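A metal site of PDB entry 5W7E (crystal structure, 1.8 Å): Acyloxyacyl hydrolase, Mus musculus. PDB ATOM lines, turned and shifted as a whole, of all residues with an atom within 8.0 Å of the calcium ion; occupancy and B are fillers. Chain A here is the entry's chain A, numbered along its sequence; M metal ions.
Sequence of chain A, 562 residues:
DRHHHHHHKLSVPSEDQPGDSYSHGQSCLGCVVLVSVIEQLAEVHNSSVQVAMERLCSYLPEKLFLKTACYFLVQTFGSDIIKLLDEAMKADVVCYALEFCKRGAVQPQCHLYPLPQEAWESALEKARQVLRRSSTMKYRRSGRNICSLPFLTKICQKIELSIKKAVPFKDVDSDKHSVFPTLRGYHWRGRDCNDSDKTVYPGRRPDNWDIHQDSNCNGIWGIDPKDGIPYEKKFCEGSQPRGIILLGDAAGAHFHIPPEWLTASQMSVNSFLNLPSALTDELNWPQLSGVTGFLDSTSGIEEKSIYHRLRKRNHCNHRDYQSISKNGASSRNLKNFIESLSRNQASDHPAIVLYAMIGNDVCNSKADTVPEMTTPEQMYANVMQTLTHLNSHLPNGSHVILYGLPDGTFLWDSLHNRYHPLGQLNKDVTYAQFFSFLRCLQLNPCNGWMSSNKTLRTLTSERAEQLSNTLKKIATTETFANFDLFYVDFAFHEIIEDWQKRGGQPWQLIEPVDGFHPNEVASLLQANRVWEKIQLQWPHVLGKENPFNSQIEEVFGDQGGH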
ATOM      1  N   CYS A 193      24.138 -18.906   3.250  1.00  0.00           N
ATOM      2  CA  CYS A 193      23.963 -17.678   4.013  1.00  0.00           C
ATOM      3  C   CYS A 193      25.044 -17.502   5.084  1.00  0.00           C
ATOM      4  O   CYS A 193      25.311 -16.364   5.507  1.00  0.00           O
ATOM      5  CB  CYS A 193      22.548 -17.613   4.635  1.00  0.00           C
ATOM      6  SG  CYS A 193      21.923 -19.082   5.573  1.00  0.00           S
ATOM      7  N   ARG A 204      18.084 -27.385   5.391  1.00  0.00           N
ATOM      8  CA  ARG A 204      18.153 -27.793   6.788  1.00  0.00           C
ATOM      9  C   ARG A 204      16.824 -27.558   7.495  1.00  0.00           C
ATOM     10  O   ARG A 204      16.157 -26.536   7.269  1.00  0.00           O
ATOM     11  CB  ARG A 204      19.272 -27.004   7.461  1.00  0.00           C
ATOM     12  CG  ARG A 204      19.570 -27.358   8.912  1.00  0.00           C
ATOM     13  CD  ARG A 204      20.950 -27.961   9.032  1.00  0.00           C
ATOM     14  NE  ARG A 204      21.304 -28.272  10.411  1.00  0.00           N
ATOM     15  CZ  ARG A 204      22.112 -29.270  10.773  1.00  0.00           C
ATOM     16  NH1 ARG A 204      22.648 -30.067   9.861  1.00  0.00           N
ATOM     17  NH2 ARG A 204      22.374 -29.482  12.061  1.00  0.00           N
ATOM     18  N   ARG A 205      16.430 -28.490   8.352  1.00  0.00           N
ATOM     19  CA  ARG A 205      15.362 -28.201   9.301  1.00  0.00           C
ATOM     20  C   ARG A 205      15.827 -27.110  10.255  1.00  0.00           C
ATOM     21  O   ARG A 205      16.964 -27.161  10.736  1.00  0.00           O
ATOM     22  CB  ARG A 205      14.967 -29.455  10.070  1.00  0.00           C
ATOM     23  CG  ARG A 205      13.950 -30.332   9.349  1.00  0.00           C
ATOM     24  CD  ARG A 205      13.057 -31.105  10.307  1.00  0.00           C
ATOM     25  NE  ARG A 205      13.863 -31.873  11.252  1.00  0.00           N
ATOM     26  CZ  ARG A 205      14.435 -33.035  10.980  1.00  0.00           C
ATOM     27  NH1 ARG A 205      14.271 -33.591   9.788  1.00  0.00           N
ATOM     28  NH2 ARG A 205      15.159 -33.650  11.899  1.00  0.00           N
ATOM     29  N   PRO A 206      15.001 -26.113  10.539  1.00  0.00           N
ATOM     30  CA  PRO A 206      15.488 -24.926  11.256  1.00  0.00           C
ATOM     31  C   PRO A 206      15.872 -25.247  12.689  1.00  0.00           C
ATOM     32  O   PRO A 206      15.073 -25.794  13.450  1.00  0.00           O
ATOM     33  CB  PRO A 206      14.306 -23.965  11.203  1.00  0.00           C
ATOM     34  CG  PRO A 206      13.107 -24.867  11.109  1.00  0.00           C
ATOM     35  CD  PRO A 206      13.553 -26.027  10.262  1.00  0.00           C
ATOM     36  N   ASP A 207      17.102 -24.908  13.047  1.00  0.00           N
ATOM     37  CA  ASP A 207      17.570 -25.056  14.422  1.00  0.00           C
ATOM     38  C   ASP A 207      16.847 -24.051  15.314  1.00  0.00           C
ATOM     39  O   ASP A 207      16.956 -22.835  15.125  1.00  0.00           O
ATOM     40  CB  ASP A 207      19.082 -24.837  14.487  1.00  0.00           C
ATOM     41  CG  ASP A 207      19.642 -25.021  15.892  1.00  0.00           C
ATOM     42  OD1 ASP A 207      19.810 -26.170  16.332  1.00  0.00           O
ATOM     43  OD2 ASP A 207      19.934 -23.992  16.556  1.00  0.00           O
ATOM     44  N   TRP A 209      13.792 -23.203  15.531  1.00  0.00           N
ATOM     45  CA  TRP A 209      12.856 -22.378  14.773  1.00  0.00           C
ATOM     46  C   TRP A 209      13.481 -21.050  14.343  1.00  0.00           C
ATOM     47  O   TRP A 209      12.784 -20.067  14.106  1.00  0.00           O
ATOM     48  CB  TRP A 209      11.564 -22.145  15.576  1.00  0.00           C
ATOM     49  CG  TRP A 209      10.675 -23.377  15.655  1.00  0.00           C
ATOM     50  CD1 TRP A 209      10.302 -24.037  16.785  1.00  0.00           C
ATOM     51  CD2 TRP A 209      10.074 -24.092  14.554  1.00  0.00           C
ATOM     52  NE1 TRP A 209       9.500 -25.114  16.464  1.00  0.00           N
ATOM     53  CE2 TRP A 209       9.353 -25.165  15.103  1.00  0.00           C
ATOM     54  CE3 TRP A 209      10.084 -23.918  13.166  1.00  0.00           C
ATOM     55  CZ2 TRP A 209       8.638 -26.065  14.306  1.00  0.00           C
ATOM     56  CZ3 TRP A 209       9.373 -24.814  12.377  1.00  0.00           C
ATOM     57  CH2 TRP A 209       8.653 -25.871  12.954  1.00  0.00           C
ATOM     58  N   ASP A 210      14.811 -21.025  14.213  1.00  0.00           N
ATOM     59  CA  ASP A 210      15.525 -19.895  13.622  1.00  0.00           C
ATOM     60  C   ASP A 210      15.252 -18.593  14.363  1.00  0.00           C
ATOM     61  O   ASP A 210      15.110 -17.525  13.760  1.00  0.00           O
ATOM     62  CB  ASP A 210      15.177 -19.770  12.138  1.00  0.00           C
ATOM     63  CG  ASP A 210      15.919 -20.769  11.270  1.00  0.00           C
ATOM     64  OD1 ASP A 210      16.663 -21.614  11.829  1.00  0.00           O
ATOM     65  OD2 ASP A 210      15.768 -20.712  10.018  1.00  0.00           O
ATOM     66  N   ILE A 211      15.204 -18.671  15.693  1.00  0.00           N
ATOM     67  CA  ILE A 211      14.970 -17.491  16.506  1.00  0.00           C
ATOM     68  C   ILE A 211      16.121 -16.511  16.377  1.00  0.00           C
ATOM     69  O   ILE A 211      15.914 -15.298  16.247  1.00  0.00           O
ATOM     70  CB  ILE A 211      14.752 -17.904  17.972  1.00  0.00           C
ATOM     71  CG1 ILE A 211      13.418 -18.631  18.118  1.00  0.00           C
ATOM     72  CG2 ILE A 211      14.802 -16.697  18.886  1.00  0.00           C
ATOM     73  CD1 ILE A 211      13.407 -19.669  19.197  1.00  0.00           C
ATOM     74  N   GLN A 213      19.143 -17.160  14.278  1.00  0.00           N
ATOM     75  CA  GLN A 213      19.831 -17.176  12.998  1.00  0.00           C
ATOM     76  C   GLN A 213      18.957 -17.870  11.969  1.00  0.00           C
ATOM     77  O   GLN A 213      18.175 -18.772  12.288  1.00  0.00           O
ATOM     78  CB  GLN A 213      21.194 -17.887  13.099  1.00  0.00           C
ATOM     79  CG  GLN A 213      21.983 -17.778  11.790  1.00  0.00           C
ATOM     80  CD  GLN A 213      23.418 -18.296  11.869  1.00  0.00           C
ATOM     81  OE1 GLN A 213      24.222 -18.017  10.972  1.00  0.00           O
ATOM     82  NE2 GLN A 213      23.738 -19.052  12.926  1.00  0.00           N
ATOM     83  N   ASP A 214      19.090 -17.424  10.715  1.00  0.00           N
ATOM     84  CA  ASP A 214      18.441 -18.102   9.597  1.00  0.00           C
ATOM     85  C   ASP A 214      19.292 -19.309   9.196  1.00  0.00           C
ATOM     86  O   ASP A 214      20.091 -19.275   8.250  1.00  0.00           O
ATOM     87  CB  ASP A 214      18.252 -17.135   8.431  1.00  0.00           C
ATOM     88  CG  ASP A 214      17.510 -17.765   7.262  1.00  0.00           C
ATOM     89  OD1 ASP A 214      17.657 -17.246   6.139  1.00  0.00           O
ATOM     90  OD2 ASP A 214      16.782 -18.758   7.484  1.00  0.00           O
ATOM     91  N   SER A 215      19.077 -20.413   9.904  1.00  0.00           N
ATOM     92  CA  SER A 215      19.924 -21.596   9.738  1.00  0.00           C
ATOM     93  C   SER A 215      19.693 -22.337   8.420  1.00  0.00           C
ATOM     94  O   SER A 215      20.557 -23.123   8.018  1.00  0.00           O
ATOM     95  CB  SER A 215      19.738 -22.554  10.915  1.00  0.00           C
ATOM     96  OG  SER A 215      18.446 -23.163  10.876  1.00  0.00           O
ATOM     97  N   ASN A 216      18.576 -22.137   7.725  1.00  0.00           N
ATOM     98  CA  ASN A 216      18.352 -22.842   6.473  1.00  0.00           C
ATOM     99  C   ASN A 216      18.286 -21.903   5.276  1.00  0.00           C
ATOM    100  O   ASN A 216      17.840 -22.312   4.194  1.00  0.00           O
ATOM    101  CB  ASN A 216      17.090 -23.708   6.551  1.00  0.00           C
ATOM    102  CG  ASN A 216      15.880 -22.939   6.987  1.00  0.00           C
ATOM    103  OD1 ASN A 216      15.894 -21.721   7.073  1.00  0.00           O
ATOM    104  ND2 ASN A 216      14.801 -23.677   7.258  1.00  0.00           N
ATOM    105  N   CYS A 217      18.722 -20.662   5.435  1.00  0.00           N
ATOM    106  CA  CYS A 217      18.957 -19.737   4.327  1.00  0.00           C
ATOM    107  C   CYS A 217      17.717 -19.399   3.524  1.00  0.00           C
ATOM    108  O   CYS A 217      17.825 -18.901   2.397  1.00  0.00           O
ATOM    109  CB  CYS A 217      20.033 -20.283   3.378  1.00  0.00           C
ATOM    110  SG  CYS A 217      21.570 -20.654   4.219  1.00  0.00           S
ATOM    111  N   ASN A 218      16.519 -19.656   4.046  1.00  0.00           N
ATOM    112  CA  ASN A 218      15.303 -19.318   3.331  1.00  0.00           C
ATOM    113  C   ASN A 218      14.822 -17.894   3.620  1.00  0.00           C
ATOM    114  O   ASN A 218      13.726 -17.528   3.181  1.00  0.00           O
ATOM    115  CB  ASN A 218      14.203 -20.337   3.621  1.00  0.00           C
ATOM    116  CG  ASN A 218      13.743 -20.314   5.060  1.00  0.00           C
ATOM    117  OD1 ASN A 218      14.194 -19.521   5.855  1.00  0.00           O
ATOM    118  ND2 ASN A 218      12.800 -21.182   5.377  1.00  0.00           N
ATOM    119  N   GLY A 219      15.621 -17.099   4.323  1.00  0.00           N
ATOM    120  CA  GLY A 219      15.312 -15.701   4.551  1.00  0.00           C
ATOM    121  C   GLY A 219      14.355 -15.437   5.682  1.00  0.00           C
ATOM    122  O   GLY A 219      14.104 -14.274   6.009  1.00  0.00           O
ATOM    123  N   ILE A 220      13.805 -16.478   6.292  1.00  0.00           N
ATOM    124  CA  ILE A 220      12.808 -16.385   7.349  1.00  0.00           C
ATOM    125  C   ILE A 220      13.503 -16.711   8.665  1.00  0.00           C
ATOM    126  O   ILE A 220      14.145 -17.762   8.780  1.00  0.00           O
ATOM    127  CB  ILE A 220      11.632 -17.331   7.086  1.00  0.00           C
ATOM    128  CG1 ILE A 220      10.994 -17.052   5.711  1.00  0.00           C
ATOM    129  CG2 ILE A 220      10.616 -17.249   8.212  1.00  0.00           C
ATOM    130  CD1 ILE A 220       9.986 -18.061   5.293  1.00  0.00           C
ATOM    131  N   TRP A 221      13.383 -15.817   9.638  1.00  0.00           N
ATOM    132  CA  TRP A 221      13.998 -16.027  10.948  1.00  0.00           C
ATOM    133  C   TRP A 221      13.484 -14.946  11.892  1.00  0.00           C
ATOM    134  O   TRP A 221      12.720 -14.057  11.489  1.00  0.00           O
ATOM    135  CB  TRP A 221      15.526 -16.000  10.867  1.00  0.00           C
ATOM    136  CG  TRP A 221      16.078 -14.633  10.600  1.00  0.00           C
ATOM    137  CD1 TRP A 221      16.071 -13.960   9.417  1.00  0.00           C
ATOM    138  CD2 TRP A 221      16.703 -13.762  11.558  1.00  0.00           C
ATOM    139  NE1 TRP A 221      16.654 -12.725   9.570  1.00  0.00           N
ATOM    140  CE2 TRP A 221      17.066 -12.582  10.876  1.00  0.00           C
ATOM    141  CE3 TRP A 221      17.011 -13.875  12.917  1.00  0.00           C
ATOM    142  CZ2 TRP A 221      17.697 -11.527  11.505  1.00  0.00           C
ATOM    143  CZ3 TRP A 221      17.636 -12.813  13.546  1.00  0.00           C
ATOM    144  CH2 TRP A 221      17.975 -11.655  12.839  1.00  0.00           C
ATOM    145  N   GLY A 222      13.922 -15.008  13.145  1.00  0.00           N
ATOM    146  CA  GLY A 222      13.507 -14.037  14.132  1.00  0.00           C
ATOM    147  C   GLY A 222      12.144 -14.381  14.698  1.00  0.00           C
ATOM    148  O   GLY A 222      11.540 -15.406  14.386  1.00  0.00           O
ATOM    149  N   TYR A 231       8.973 -16.595  13.493  1.00  0.00           N
ATOM    150  CA  TYR A 231       8.363 -16.486  12.173  1.00  0.00           C
ATOM    151  C   TYR A 231       8.431 -17.807  11.410  1.00  0.00           C
ATOM    152  O   TYR A 231       7.484 -18.174  10.718  1.00  0.00           O
ATOM    153  CB  TYR A 231       9.060 -15.383  11.388  1.00  0.00           C
ATOM    154  CG  TYR A 231       8.626 -13.979  11.739  1.00  0.00           C
ATOM    155  CD1 TYR A 231       9.549 -13.040  12.196  1.00  0.00           C
ATOM    156  CD2 TYR A 231       7.309 -13.575  11.591  1.00  0.00           C
ATOM    157  CE1 TYR A 231       9.172 -11.749  12.499  1.00  0.00           C
ATOM    158  CE2 TYR A 231       6.915 -12.285  11.892  1.00  0.00           C
ATOM    159  CZ  TYR A 231       7.847 -11.379  12.350  1.00  0.00           C
ATOM    160  OH  TYR A 231       7.450 -10.106  12.636  1.00  0.00           O
ATOM    161  N   GLU A 232       9.549 -18.517  11.514  1.00  0.00           N
ATOM    162  CA  GLU A 232       9.665 -19.781  10.793  1.00  0.00           C
ATOM    163  C   GLU A 232       8.678 -20.805  11.330  1.00  0.00           C
ATOM    164  O   GLU A 232       8.137 -21.619  10.574  1.00  0.00           O
ATOM    165  CB  GLU A 232      11.106 -20.294  10.866  1.00  0.00           C
ATOM    166  CG  GLU A 232      11.332 -21.646  10.168  1.00  0.00           C
ATOM    167  CD  GLU A 232      12.206 -21.620   8.909  1.00  0.00           C
ATOM    168  OE1 GLU A 232      12.113 -22.579   8.125  1.00  0.00           O
ATOM    169  OE2 GLU A 232      12.997 -20.678   8.691  1.00  0.00           O
ATOM    170  N   CYS A 236       6.095 -21.555   8.563  1.00  0.00           N
ATOM    171  CA  CYS A 236       6.569 -22.773   7.888  1.00  0.00           C
ATOM    172  C   CYS A 236       6.207 -24.096   8.574  1.00  0.00           C
ATOM    173  O   CYS A 236       6.175 -25.116   7.880  1.00  0.00           O
ATOM    174  CB  CYS A 236       8.094 -22.741   7.728  1.00  0.00           C
ATOM    175  SG  CYS A 236       8.664 -21.366   6.682  1.00  0.00           S
ATOM    176  N   CYS A 316       8.706 -21.016   1.910  1.00  0.00           N
ATOM    177  CA  CYS A 316       9.693 -21.577   2.822  1.00  0.00           C
ATOM    178  C   CYS A 316      10.800 -22.322   2.085  1.00  0.00           C
ATOM    179  O   CYS A 316      11.873 -22.527   2.653  1.00  0.00           O
ATOM    180  CB  CYS A 316       9.036 -22.541   3.828  1.00  0.00           C
ATOM    181  SG  CYS A 316       7.796 -21.736   4.831  1.00  0.00           S
ATOM    182  N   HIS A 318      12.554 -21.286  -0.391  1.00  0.00           N
ATOM    183  CA  HIS A 318      13.548 -20.375  -0.958  1.00  0.00           C
ATOM    184  C   HIS A 318      14.969 -20.913  -0.782  1.00  0.00           C
ATOM    185  O   HIS A 318      15.409 -21.219   0.336  1.00  0.00           O
ATOM    186  CB  HIS A 318      13.388 -19.007  -0.296  1.00  0.00           C
ATOM    187  CG  HIS A 318      14.353 -17.986  -0.792  1.00  0.00           C
ATOM    188  ND1 HIS A 318      14.341 -17.508  -2.081  1.00  0.00           N
ATOM    189  CD2 HIS A 318      15.368 -17.341  -0.170  1.00  0.00           C
ATOM    190  CE1 HIS A 318      15.304 -16.612  -2.232  1.00  0.00           C
ATOM    191  NE2 HIS A 318      15.940 -16.497  -1.082  1.00  0.00           N
ATOM    192  N   PHE A 556       9.413 -10.276   4.984  1.00  0.00           N
ATOM    193  CA  PHE A 556      10.766 -10.580   4.548  1.00  0.00           C
ATOM    194  C   PHE A 556      11.054 -10.197   3.096  1.00  0.00           C
ATOM    195  O   PHE A 556      12.185 -10.390   2.625  1.00  0.00           O
ATOM    196  CB  PHE A 556      11.063 -12.080   4.736  1.00  0.00           C
ATOM    197  CG  PHE A 556      10.922 -12.563   6.158  1.00  0.00           C
ATOM    198  CD1 PHE A 556      11.919 -12.323   7.087  1.00  0.00           C
ATOM    199  CD2 PHE A 556       9.797 -13.266   6.554  1.00  0.00           C
ATOM    200  CE1 PHE A 556      11.789 -12.762   8.413  1.00  0.00           C
ATOM    201  CE2 PHE A 556       9.663 -13.709   7.872  1.00  0.00           C
ATOM    202  CZ  PHE A 556      10.664 -13.453   8.802  1.00  0.00           C
ATOM    203  N   GLN A 559      13.254 -12.285   0.649  1.00  0.00           N
ATOM    204  CA  GLN A 559      13.826 -13.352   1.475  1.00  0.00           C
ATOM    205  C   GLN A 559      15.342 -13.473   1.317  1.00  0.00           C
ATOM    206  O   GLN A 559      15.932 -14.536   1.548  1.00  0.00           O
ATOM    207  CB  GLN A 559      13.146 -14.693   1.181  1.00  0.00           C
ATOM    208  CG  GLN A 559      11.707 -14.710   1.670  1.00  0.00           C
ATOM    209  CD  GLN A 559      10.942 -15.934   1.242  1.00  0.00           C
ATOM    210  OE1 GLN A 559      10.064 -15.856   0.385  1.00  0.00           O
ATOM    211  NE2 GLN A 559      11.254 -17.067   1.833  1.00  0.00           N
HETATM  212 CA    CA M   1      14.948 -19.833   8.073  1.00  0.00          CA
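The calcium ion is bound by the side-chain carboxylate of Asp 214 (2.2 Å), the side-chain carboxylate of Glu 232 (2.2 Å), the side-chain carboxylate of Asp 210 (2.3 Å), the backbone carbonyl oxygen of Ile 220 (2.3 Å), the side-chain amide oxygen of Asn 216 (2.3 Å) and the side-chain amide oxygen of Asn 218 (2.4 Å).
The calcium ion has six donor atoms within binding distance.
Of the 25 residues printed, 6 come within 4 Å of the calcium ion.
Along chain A the residues within 4 Å of the calcium ion span positions 210 to 232.
The nearest printed residue that does not touch the calcium ion is Ser 215 (4.6 Å).
The side-chain amide nitrogen (ND2) of Asn 216 sits close to the backbone carbonyl oxygen (O) of Arg 204, 3.2 Å away.
O of Asp 210 sits at hydrogen-bond distance from N of Gly 222 (2.9 Å).
OG of Ser 215 lies within hydrogen-bond range of OD1 of Asp 210, at 2.5 Å.
OD1 of Asp 214 lies within hydrogen-bond range of N of Gly 219, at 2.7 Å.
The side-chain sulfur of Cys 217 forms a disulfide with the side-chain sulfur of Cys 193.
The backbone carbonyl oxygen (O) of Asn 218 sits at hydrogen-bond distance from the side-chain amide nitrogen (NE2) of Gln 559.
The side-chain amide nitrogen of Asn 218 lies within hydrogen-bond range of the backbone carbonyl oxygen of Cys 316.
The side-chain carboxylate (OD2) of Asp 214 lies close to the backbone NH (N) of Cys 217, 3.4 Å away.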
